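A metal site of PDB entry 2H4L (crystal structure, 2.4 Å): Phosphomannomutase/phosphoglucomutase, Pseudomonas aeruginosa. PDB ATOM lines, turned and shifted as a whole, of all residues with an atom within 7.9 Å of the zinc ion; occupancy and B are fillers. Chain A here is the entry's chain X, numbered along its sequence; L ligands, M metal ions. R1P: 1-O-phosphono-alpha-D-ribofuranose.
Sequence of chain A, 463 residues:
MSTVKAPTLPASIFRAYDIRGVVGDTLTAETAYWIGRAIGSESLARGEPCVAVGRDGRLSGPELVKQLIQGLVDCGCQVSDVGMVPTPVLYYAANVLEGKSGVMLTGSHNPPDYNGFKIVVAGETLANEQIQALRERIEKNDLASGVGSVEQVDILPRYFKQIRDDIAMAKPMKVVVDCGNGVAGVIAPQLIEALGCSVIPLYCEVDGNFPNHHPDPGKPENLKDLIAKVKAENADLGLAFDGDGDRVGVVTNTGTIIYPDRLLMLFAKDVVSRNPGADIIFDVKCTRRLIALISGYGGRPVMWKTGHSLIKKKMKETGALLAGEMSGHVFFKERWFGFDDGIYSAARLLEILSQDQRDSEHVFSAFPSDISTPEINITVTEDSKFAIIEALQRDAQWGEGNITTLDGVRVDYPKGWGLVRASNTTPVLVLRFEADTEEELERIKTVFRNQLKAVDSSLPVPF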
ATOM      1  N   ARG A  20      29.093  -3.738 -14.019  1.00  0.00           N
ATOM      2  CA  ARG A  20      29.766  -2.437 -13.961  1.00  0.00           C
ATOM      3  C   ARG A  20      31.208  -2.522 -14.457  1.00  0.00           C
ATOM      4  O   ARG A  20      32.044  -3.166 -13.844  1.00  0.00           O
ATOM      5  CB  ARG A  20      29.716  -1.881 -12.531  1.00  0.00           C
ATOM      6  CG  ARG A  20      28.427  -1.107 -12.230  1.00  0.00           C
ATOM      7  CD  ARG A  20      28.163  -0.886 -10.749  1.00  0.00           C
ATOM      8  NE  ARG A  20      26.718  -0.858 -10.530  1.00  0.00           N
ATOM      9  CZ  ARG A  20      25.994   0.211 -10.180  1.00  0.00           C
ATOM     10  NH1 ARG A  20      26.562   1.386  -9.942  1.00  0.00           N
ATOM     11  NH2 ARG A  20      24.667   0.087 -10.053  1.00  0.00           N
ATOM     12  N   ARG A  58      26.513   8.553 -22.241  1.00  0.00           N
ATOM     13  CA  ARG A  58      27.966   8.347 -22.181  1.00  0.00           C
ATOM     14  C   ARG A  58      28.580   8.270 -23.578  1.00  0.00           C
ATOM     15  O   ARG A  58      27.892   7.972 -24.559  1.00  0.00           O
ATOM     16  CB  ARG A  58      28.305   7.116 -21.324  1.00  0.00           C
ATOM     17  CG  ARG A  58      28.396   7.472 -19.869  1.00  0.00           C
ATOM     18  CD  ARG A  58      28.092   6.355 -18.893  1.00  0.00           C
ATOM     19  NE  ARG A  58      27.740   6.946 -17.597  1.00  0.00           N
ATOM     20  CZ  ARG A  58      28.627   7.343 -16.671  1.00  0.00           C
ATOM     21  NH1 ARG A  58      29.923   7.191 -16.861  1.00  0.00           N
ATOM     22  NH2 ARG A  58      28.199   7.880 -15.545  1.00  0.00           N
ATOM     23  N   THR A  87      17.643   5.750 -17.304  1.00  0.00           N
ATOM     24  CA  THR A  87      17.480   4.371 -16.854  1.00  0.00           C
ATOM     25  C   THR A  87      15.998   4.019 -16.617  1.00  0.00           C
ATOM     26  O   THR A  87      15.523   3.018 -17.180  1.00  0.00           O
ATOM     27  CB  THR A  87      18.375   4.067 -15.611  1.00  0.00           C
ATOM     28  OG1 THR A  87      19.741   3.951 -16.028  1.00  0.00           O
ATOM     29  CG2 THR A  87      17.986   2.760 -14.950  1.00  0.00           C
ATOM     30  N   PRO A  88      15.261   4.832 -15.810  1.00  0.00           N
ATOM     31  CA  PRO A  88      13.854   4.513 -15.531  1.00  0.00           C
ATOM     32  C   PRO A  88      12.951   4.438 -16.758  1.00  0.00           C
ATOM     33  O   PRO A  88      11.937   3.725 -16.731  1.00  0.00           O
ATOM     34  CB  PRO A  88      13.411   5.664 -14.618  1.00  0.00           C
ATOM     35  CG  PRO A  88      14.400   6.750 -14.850  1.00  0.00           C
ATOM     36  CD  PRO A  88      15.683   6.034 -15.079  1.00  0.00           C
ATOM     37  N   TYR A  91      13.236   0.937 -17.927  1.00  0.00           N
ATOM     38  CA  TYR A  91      12.374   0.137 -17.053  1.00  0.00           C
ATOM     39  C   TYR A  91      10.892   0.312 -17.419  1.00  0.00           C
ATOM     40  O   TYR A  91      10.140  -0.656 -17.471  1.00  0.00           O
ATOM     41  CB  TYR A  91      12.566   0.525 -15.581  1.00  0.00           C
ATOM     42  CG  TYR A  91      13.946   0.334 -14.994  1.00  0.00           C
ATOM     43  CD1 TYR A  91      14.849  -0.601 -15.516  1.00  0.00           C
ATOM     44  CD2 TYR A  91      14.339   1.068 -13.866  1.00  0.00           C
ATOM     45  CE1 TYR A  91      16.107  -0.765 -14.946  1.00  0.00           C
ATOM     46  CE2 TYR A  91      15.573   0.906 -13.288  1.00  0.00           C
ATOM     47  CZ  TYR A  91      16.461  -0.013 -13.831  1.00  0.00           C
ATOM     48  OH  TYR A  91      17.702  -0.173 -13.246  1.00  0.00           O
ATOM     49  N   THR A 106      24.327   1.686 -19.120  1.00  0.00           N
ATOM     50  CA  THR A 106      24.654   2.898 -18.367  1.00  0.00           C
ATOM     51  C   THR A 106      25.824   2.656 -17.413  1.00  0.00           C
ATOM     52  O   THR A 106      26.027   1.538 -16.960  1.00  0.00           O
ATOM     53  CB  THR A 106      23.429   3.429 -17.560  1.00  0.00           C
ATOM     54  OG1 THR A 106      23.795   4.597 -16.846  1.00  0.00           O
ATOM     55  CG2 THR A 106      22.929   2.412 -16.539  1.00  0.00           C
ATOM     56  N   GLY A 107      26.579   3.724 -17.115  1.00  0.00           N
ATOM     57  CA  GLY A 107      27.588   3.720 -16.045  1.00  0.00           C
ATOM     58  C   GLY A 107      27.179   4.552 -14.835  1.00  0.00           C
ATOM     59  O   GLY A 107      28.035   5.138 -14.169  1.00  0.00           O
ATOM     60  N   SEP A 108      25.860   4.586 -14.571  1.00  0.00           N
ATOM     61  CA  SEP A 108      25.217   5.253 -13.422  1.00  0.00           C
ATOM     62  CB  SEP A 108      25.111   4.312 -12.168  1.00  0.00           C
ATOM     63  OG  SEP A 108      23.934   4.597 -11.369  1.00  0.00           O
ATOM     64  C   SEP A 108      25.752   6.665 -13.097  1.00  0.00           C
ATOM     65  O   SEP A 108      25.629   7.579 -13.913  1.00  0.00           O
ATOM     66  P   SEP A 108      23.875   4.009  -9.844  1.00  0.00           P
ATOM     67  O1P SEP A 108      25.343   4.054  -9.236  1.00  0.00           O
ATOM     68  O2P SEP A 108      23.311   2.497  -9.822  1.00  0.00           O
ATOM     69  O3P SEP A 108      22.869   4.800  -8.878  1.00  0.00           O
ATOM     70  N   HIS A 109      26.350   6.821 -11.915  1.00  0.00           N
ATOM     71  CA  HIS A 109      26.843   8.118 -11.419  1.00  0.00           C
ATOM     72  C   HIS A 109      28.369   8.241 -11.561  1.00  0.00           C
ATOM     73  O   HIS A 109      28.967   9.231 -11.110  1.00  0.00           O
ATOM     74  CB  HIS A 109      26.454   8.271  -9.945  1.00  0.00           C
ATOM     75  CG  HIS A 109      27.188   7.336  -9.025  1.00  0.00           C
ATOM     76  ND1 HIS A 109      26.797   6.028  -8.818  1.00  0.00           N
ATOM     77  CD2 HIS A 109      28.313   7.506  -8.288  1.00  0.00           C
ATOM     78  CE1 HIS A 109      27.635   5.437  -7.987  1.00  0.00           C
ATOM     79  NE2 HIS A 109      28.569   6.317  -7.649  1.00  0.00           N
ATOM     80  N   ASN A 110      28.982   7.232 -12.168  1.00  0.00           N
ATOM     81  CA  ASN A 110      30.450   7.115 -12.222  1.00  0.00           C
ATOM     82  C   ASN A 110      31.107   7.990 -13.290  1.00  0.00           C
ATOM     83  O   ASN A 110      30.420   8.448 -14.211  1.00  0.00           O
ATOM     84  CB  ASN A 110      30.837   5.646 -12.441  1.00  0.00           C
ATOM     85  CG  ASN A 110      30.311   4.725 -11.342  1.00  0.00           C
ATOM     86  OD1 ASN A 110      29.618   3.745 -11.619  1.00  0.00           O
ATOM     87  ND2 ASN A 110      30.646   5.024 -10.091  1.00  0.00           N
ATOM     88  N   LYS A 118      22.238  -2.565 -16.488  1.00  0.00           N
ATOM     89  CA  LYS A 118      21.163  -2.912 -15.564  1.00  0.00           C
ATOM     90  C   LYS A 118      20.141  -3.771 -16.317  1.00  0.00           C
ATOM     91  O   LYS A 118      19.697  -3.420 -17.421  1.00  0.00           O
ATOM     92  CB  LYS A 118      20.567  -1.639 -14.963  1.00  0.00           C
ATOM     93  CG  LYS A 118      21.526  -0.975 -13.968  1.00  0.00           C
ATOM     94  CD  LYS A 118      21.221   0.493 -13.715  1.00  0.00           C
ATOM     95  CE  LYS A 118      22.182   1.044 -12.660  1.00  0.00           C
ATOM     96  NZ  LYS A 118      21.989   2.493 -12.350  1.00  0.00           N
ATOM     97  N   PRO A 215      27.952  13.559 -12.125  1.00  0.00           N
ATOM     98  CA  PRO A 215      26.511  13.506 -11.906  1.00  0.00           C
ATOM     99  C   PRO A 215      26.158  12.548 -10.747  1.00  0.00           C
ATOM    100  O   PRO A 215      25.581  11.485 -10.947  1.00  0.00           O
ATOM    101  CB  PRO A 215      25.974  13.025 -13.260  1.00  0.00           C
ATOM    102  CG  PRO A 215      27.066  12.188 -13.827  1.00  0.00           C
ATOM    103  CD  PRO A 215      28.372  12.762 -13.301  1.00  0.00           C
ATOM    104  N   PRO A 217      24.435  13.133  -7.092  1.00  0.00           N
ATOM    105  CA  PRO A 217      23.779  13.954  -6.071  1.00  0.00           C
ATOM    106  C   PRO A 217      23.903  13.405  -4.634  1.00  0.00           C
ATOM    107  O   PRO A 217      23.447  14.057  -3.694  1.00  0.00           O
ATOM    108  CB  PRO A 217      22.309  13.977  -6.508  1.00  0.00           C
ATOM    109  CG  PRO A 217      22.129  12.739  -7.299  1.00  0.00           C
ATOM    110  CD  PRO A 217      23.451  12.466  -7.968  1.00  0.00           C
ATOM    111  N   PHE A 241      19.861  15.313 -10.362  1.00  0.00           N
ATOM    112  CA  PHE A 241      19.683  13.951 -10.906  1.00  0.00           C
ATOM    113  C   PHE A 241      21.057  13.373 -11.137  1.00  0.00           C
ATOM    114  O   PHE A 241      22.004  14.107 -11.436  1.00  0.00           O
ATOM    115  CB  PHE A 241      18.874  13.978 -12.214  1.00  0.00           C
ATOM    116  CG  PHE A 241      17.441  14.400 -12.023  1.00  0.00           C
ATOM    117  CD1 PHE A 241      16.489  13.471 -11.590  1.00  0.00           C
ATOM    118  CD2 PHE A 241      17.049  15.717 -12.221  1.00  0.00           C
ATOM    119  CE1 PHE A 241      15.163  13.861 -11.377  1.00  0.00           C
ATOM    120  CE2 PHE A 241      15.733  16.117 -12.007  1.00  0.00           C
ATOM    121  CZ  PHE A 241      14.790  15.190 -11.585  1.00  0.00           C
ATOM    122  N   ASP A 242      21.173  12.052 -10.963  1.00  0.00           N
ATOM    123  CA  ASP A 242      22.421  11.355 -11.268  1.00  0.00           C
ATOM    124  C   ASP A 242      22.503  11.042 -12.743  1.00  0.00           C
ATOM    125  O   ASP A 242      21.521  11.221 -13.476  1.00  0.00           O
ATOM    126  CB  ASP A 242      22.574  10.074 -10.420  1.00  0.00           C
ATOM    127  CG  ASP A 242      21.785   8.899 -10.955  1.00  0.00           C
ATOM    128  OD1 ASP A 242      20.688   9.098 -11.512  1.00  0.00           O
ATOM    129  OD2 ASP A 242      22.258   7.769 -10.770  1.00  0.00           O
ATOM    130  N   GLY A 243      23.662  10.558 -13.165  1.00  0.00           N
ATOM    131  CA  GLY A 243      23.932  10.251 -14.570  1.00  0.00           C
ATOM    132  C   GLY A 243      22.766   9.670 -15.364  1.00  0.00           C
ATOM    133  O   GLY A 243      22.418  10.181 -16.424  1.00  0.00           O
ATOM    134  N   ASP A 244      22.187   8.594 -14.857  1.00  0.00           N
ATOM    135  CA  ASP A 244      21.168   7.847 -15.616  1.00  0.00           C
ATOM    136  C   ASP A 244      19.736   8.130 -15.183  1.00  0.00           C
ATOM    137  O   ASP A 244      18.780   7.603 -15.784  1.00  0.00           O
ATOM    138  CB  ASP A 244      21.488   6.340 -15.626  1.00  0.00           C
ATOM    139  CG  ASP A 244      21.564   5.713 -14.227  1.00  0.00           C
ATOM    140  OD1 ASP A 244      21.818   6.429 -13.233  1.00  0.00           O
ATOM    141  OD2 ASP A 244      21.403   4.479 -14.129  1.00  0.00           O
ATOM    142  N   GLY A 245      19.578   8.962 -14.150  1.00  0.00           N
ATOM    143  CA  GLY A 245      18.264   9.465 -13.738  1.00  0.00           C
ATOM    144  C   GLY A 245      17.451   8.568 -12.799  1.00  0.00           C
ATOM    145  O   GLY A 245      16.239   8.789 -12.620  1.00  0.00           O
ATOM    146  N   ASP A 246      18.100   7.577 -12.191  1.00  0.00           N
ATOM    147  CA  ASP A 246      17.408   6.712 -11.227  1.00  0.00           C
ATOM    148  C   ASP A 246      17.591   7.177  -9.778  1.00  0.00           C
ATOM    149  O   ASP A 246      16.998   6.619  -8.866  1.00  0.00           O
ATOM    150  CB  ASP A 246      17.758   5.218 -11.426  1.00  0.00           C
ATOM    151  CG  ASP A 246      19.240   4.932 -11.287  1.00  0.00           C
ATOM    152  OD1 ASP A 246      20.043   5.840 -11.020  1.00  0.00           O
ATOM    153  OD2 ASP A 246      19.601   3.734 -11.455  1.00  0.00           O
ATOM    154  N   ARG A 247      18.402   8.228  -9.594  1.00  0.00           N
ATOM    155  CA  ARG A 247      18.591   8.859  -8.283  1.00  0.00           C
ATOM    156  C   ARG A 247      18.187  10.330  -8.305  1.00  0.00           C
ATOM    157  O   ARG A 247      18.436  11.036  -9.294  1.00  0.00           O
ATOM    158  CB  ARG A 247      20.041   8.748  -7.849  1.00  0.00           C
ATOM    159  CG  ARG A 247      20.563   7.348  -7.769  1.00  0.00           C
ATOM    160  CD  ARG A 247      21.516   7.179  -6.615  1.00  0.00           C
ATOM    161  NE  ARG A 247      22.566   8.192  -6.579  1.00  0.00           N
ATOM    162  CZ  ARG A 247      23.755   8.036  -7.156  1.00  0.00           C
ATOM    163  NH1 ARG A 247      24.045   6.924  -7.817  1.00  0.00           N
ATOM    164  NH2 ARG A 247      24.664   9.003  -7.071  1.00  0.00           N
ATOM    165  N   VAL A 248      17.579  10.794  -7.216  1.00  0.00           N
ATOM    166  CA  VAL A 248      17.247  12.208  -7.062  1.00  0.00           C
ATOM    167  C   VAL A 248      17.816  12.826  -5.770  1.00  0.00           C
ATOM    168  O   VAL A 248      17.836  12.186  -4.715  1.00  0.00           O
ATOM    169  CB  VAL A 248      15.700  12.467  -7.196  1.00  0.00           C
ATOM    170  CG1 VAL A 248      14.931  11.928  -5.999  1.00  0.00           C
ATOM    171  CG2 VAL A 248      15.419  13.950  -7.401  1.00  0.00           C
ATOM    172  N   HIS A 308      19.461  -1.410  -5.644  1.00  0.00           N
ATOM    173  CA  HIS A 308      18.221  -1.260  -6.408  1.00  0.00           C
ATOM    174  C   HIS A 308      17.524  -2.577  -6.783  1.00  0.00           C
ATOM    175  O   HIS A 308      16.314  -2.705  -6.612  1.00  0.00           O
ATOM    176  CB  HIS A 308      18.441  -0.349  -7.635  1.00  0.00           C
ATOM    177  CG  HIS A 308      19.281  -0.971  -8.708  1.00  0.00           C
ATOM    178  ND1 HIS A 308      18.733  -1.581  -9.828  1.00  0.00           N
ATOM    179  CD2 HIS A 308      20.624  -1.102  -8.835  1.00  0.00           C
ATOM    180  CE1 HIS A 308      19.701  -2.051 -10.584  1.00  0.00           C
ATOM    181  NE2 HIS A 308      20.861  -1.769 -10.007  1.00  0.00           N
ATOM    182  N   SER A 327      20.866   6.099  -0.863  1.00  0.00           N
ATOM    183  CA  SER A 327      21.585   6.587  -2.046  1.00  0.00           C
ATOM    184  C   SER A 327      20.765   7.550  -2.932  1.00  0.00           C
ATOM    185  O   SER A 327      21.355   8.332  -3.677  1.00  0.00           O
ATOM    186  CB  SER A 327      22.067   5.416  -2.918  1.00  0.00           C
ATOM    187  OG  SER A 327      20.966   4.670  -3.408  1.00  0.00           O
ATOM    188  N   HIS A 329      17.688   6.336  -4.572  1.00  0.00           N
ATOM    189  CA  HIS A 329      16.771   5.536  -5.356  1.00  0.00           C
ATOM    190  C   HIS A 329      15.438   5.535  -4.637  1.00  0.00           C
ATOM    191  O   HIS A 329      15.387   5.259  -3.432  1.00  0.00           O
ATOM    192  CB  HIS A 329      17.277   4.107  -5.522  1.00  0.00           C
ATOM    193  CG  HIS A 329      18.493   3.983  -6.383  1.00  0.00           C
ATOM    194  ND1 HIS A 329      18.429   3.574  -7.709  1.00  0.00           N
ATOM    195  CD2 HIS A 329      19.801   4.206  -6.121  1.00  0.00           C
ATOM    196  CE1 HIS A 329      19.651   3.547  -8.207  1.00  0.00           C
ATOM    197  NE2 HIS A 329      20.502   3.928  -7.268  1.00  0.00           N
ATOM    198  N   ASP A 340      12.739   2.096  -9.556  1.00  0.00           N
ATOM    199  CA  ASP A 340      13.342   3.341  -9.096  1.00  0.00           C
ATOM    200  C   ASP A 340      13.349   4.329 -10.249  1.00  0.00           C
ATOM    201  O   ASP A 340      13.650   3.967 -11.390  1.00  0.00           O
ATOM    202  CB  ASP A 340      14.768   3.139  -8.537  1.00  0.00           C
ATOM    203  CG  ASP A 340      15.611   2.142  -9.349  1.00  0.00           C
ATOM    204  OD1 ASP A 340      15.064   1.115  -9.809  1.00  0.00           O
ATOM    205  OD2 ASP A 340      16.836   2.380  -9.507  1.00  0.00           O
HETATM  206  C5  R1P L   1      24.422   1.581  -6.697  1.00  0.00           C
HETATM  207  O5  R1P L   1      23.276   1.051  -7.351  1.00  0.00           O
HETATM  208  C4  R1P L   1      24.364   1.142  -5.250  1.00  0.00           C
HETATM  209  O4  R1P L   1      25.677   0.930  -4.735  1.00  0.00           O
HETATM  210  C1  R1P L   1      25.921   1.683  -3.563  1.00  0.00           C
HETATM  211  C2  R1P L   1      24.711   2.572  -3.318  1.00  0.00           C
HETATM  212  O2  R1P L   1      24.193   2.477  -1.997  1.00  0.00           O
HETATM  213  C3  R1P L   1      23.688   2.173  -4.372  1.00  0.00           C
HETATM  214  O3  R1P L   1      22.620   1.502  -3.742  1.00  0.00           O
HETATM  215  O1  R1P L   1      25.821   0.666  -2.572  1.00  0.00           O
HETATM  216  P   R1P L   1      27.055  -0.179  -1.995  1.00  0.00           P
HETATM  217  O1P R1P L   1      26.611  -1.700  -1.899  1.00  0.00           O
HETATM  218  O2P R1P L   1      28.352  -0.029  -2.891  1.00  0.00           O
HETATM  219  O3P R1P L   1      27.400   0.387  -0.548  1.00  0.00           O
HETATM  220 ZN    ZN M   1      21.957   6.070 -11.193  1.00  0.00          ZN
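O2P of SEP 108 sits at hydrogen-bond distance from O5 of the ligand.
O5 of the ligand sits at hydrogen-bond distance from NH2 of Arg 20.
Lys 118 touches the zinc ion.
Arg 247 touches the zinc ion (CG to ZN, 3.9 Å).
Six residues have an atom within 4 Å of the zinc ion: SEP 108, Lys 118, Asp 242, Asp 244, Asp 246 and Arg 247.
The nearest printed residue that does not touch the zinc ion is His 109 (4.5 Å).
The zinc ion is bound by the side-chain carboxylate (OD2) of Asp 242 (1.8 Å), the side-chain carboxylate (OD1) of Asp 246 (1.9 Å), the side-chain carboxylate (OD1) of Asp 244 (2.1 Å) and OG of SEP 108 (2.5 Å).
The zinc ion has four donor atoms within binding distance.
Slightly farther from the zinc ion lies O3P of SEP 108 (2.8 Å).
N of Arg 247 lies within hydrogen-bond range of OD1 of Asp 242 (3.1 Å).
The side-chain amino group of Lys 118 lies within salt-bridge range of the side-chain carboxylate of Asp 246, at 2.8 Å.
OD2 of Asp 244 lies within salt-bridge range of NZ of Lys 118, at 2.7 Å.
OD2 of Asp 244 is in hydrogen-bond range of OG1 of Thr 87 (2.6 Å).
The side-chain amino group of Lys 118 lies within salt-bridge range of O2P of SEP 108 (2.9 Å).
O3P of SEP 108 sits at hydrogen-bond distance from a ring nitrogen (NE2) of His 329, 3.0 Å away.
NH2 of Arg 20 is in salt-bridge range of O2P of SEP 108, at 2.8 Å.
The backbone carbonyl oxygen (O) of Ser 327 sits at hydrogen-bond distance from the guanidinium group (NE) of Arg 247, 3.1 Å away.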
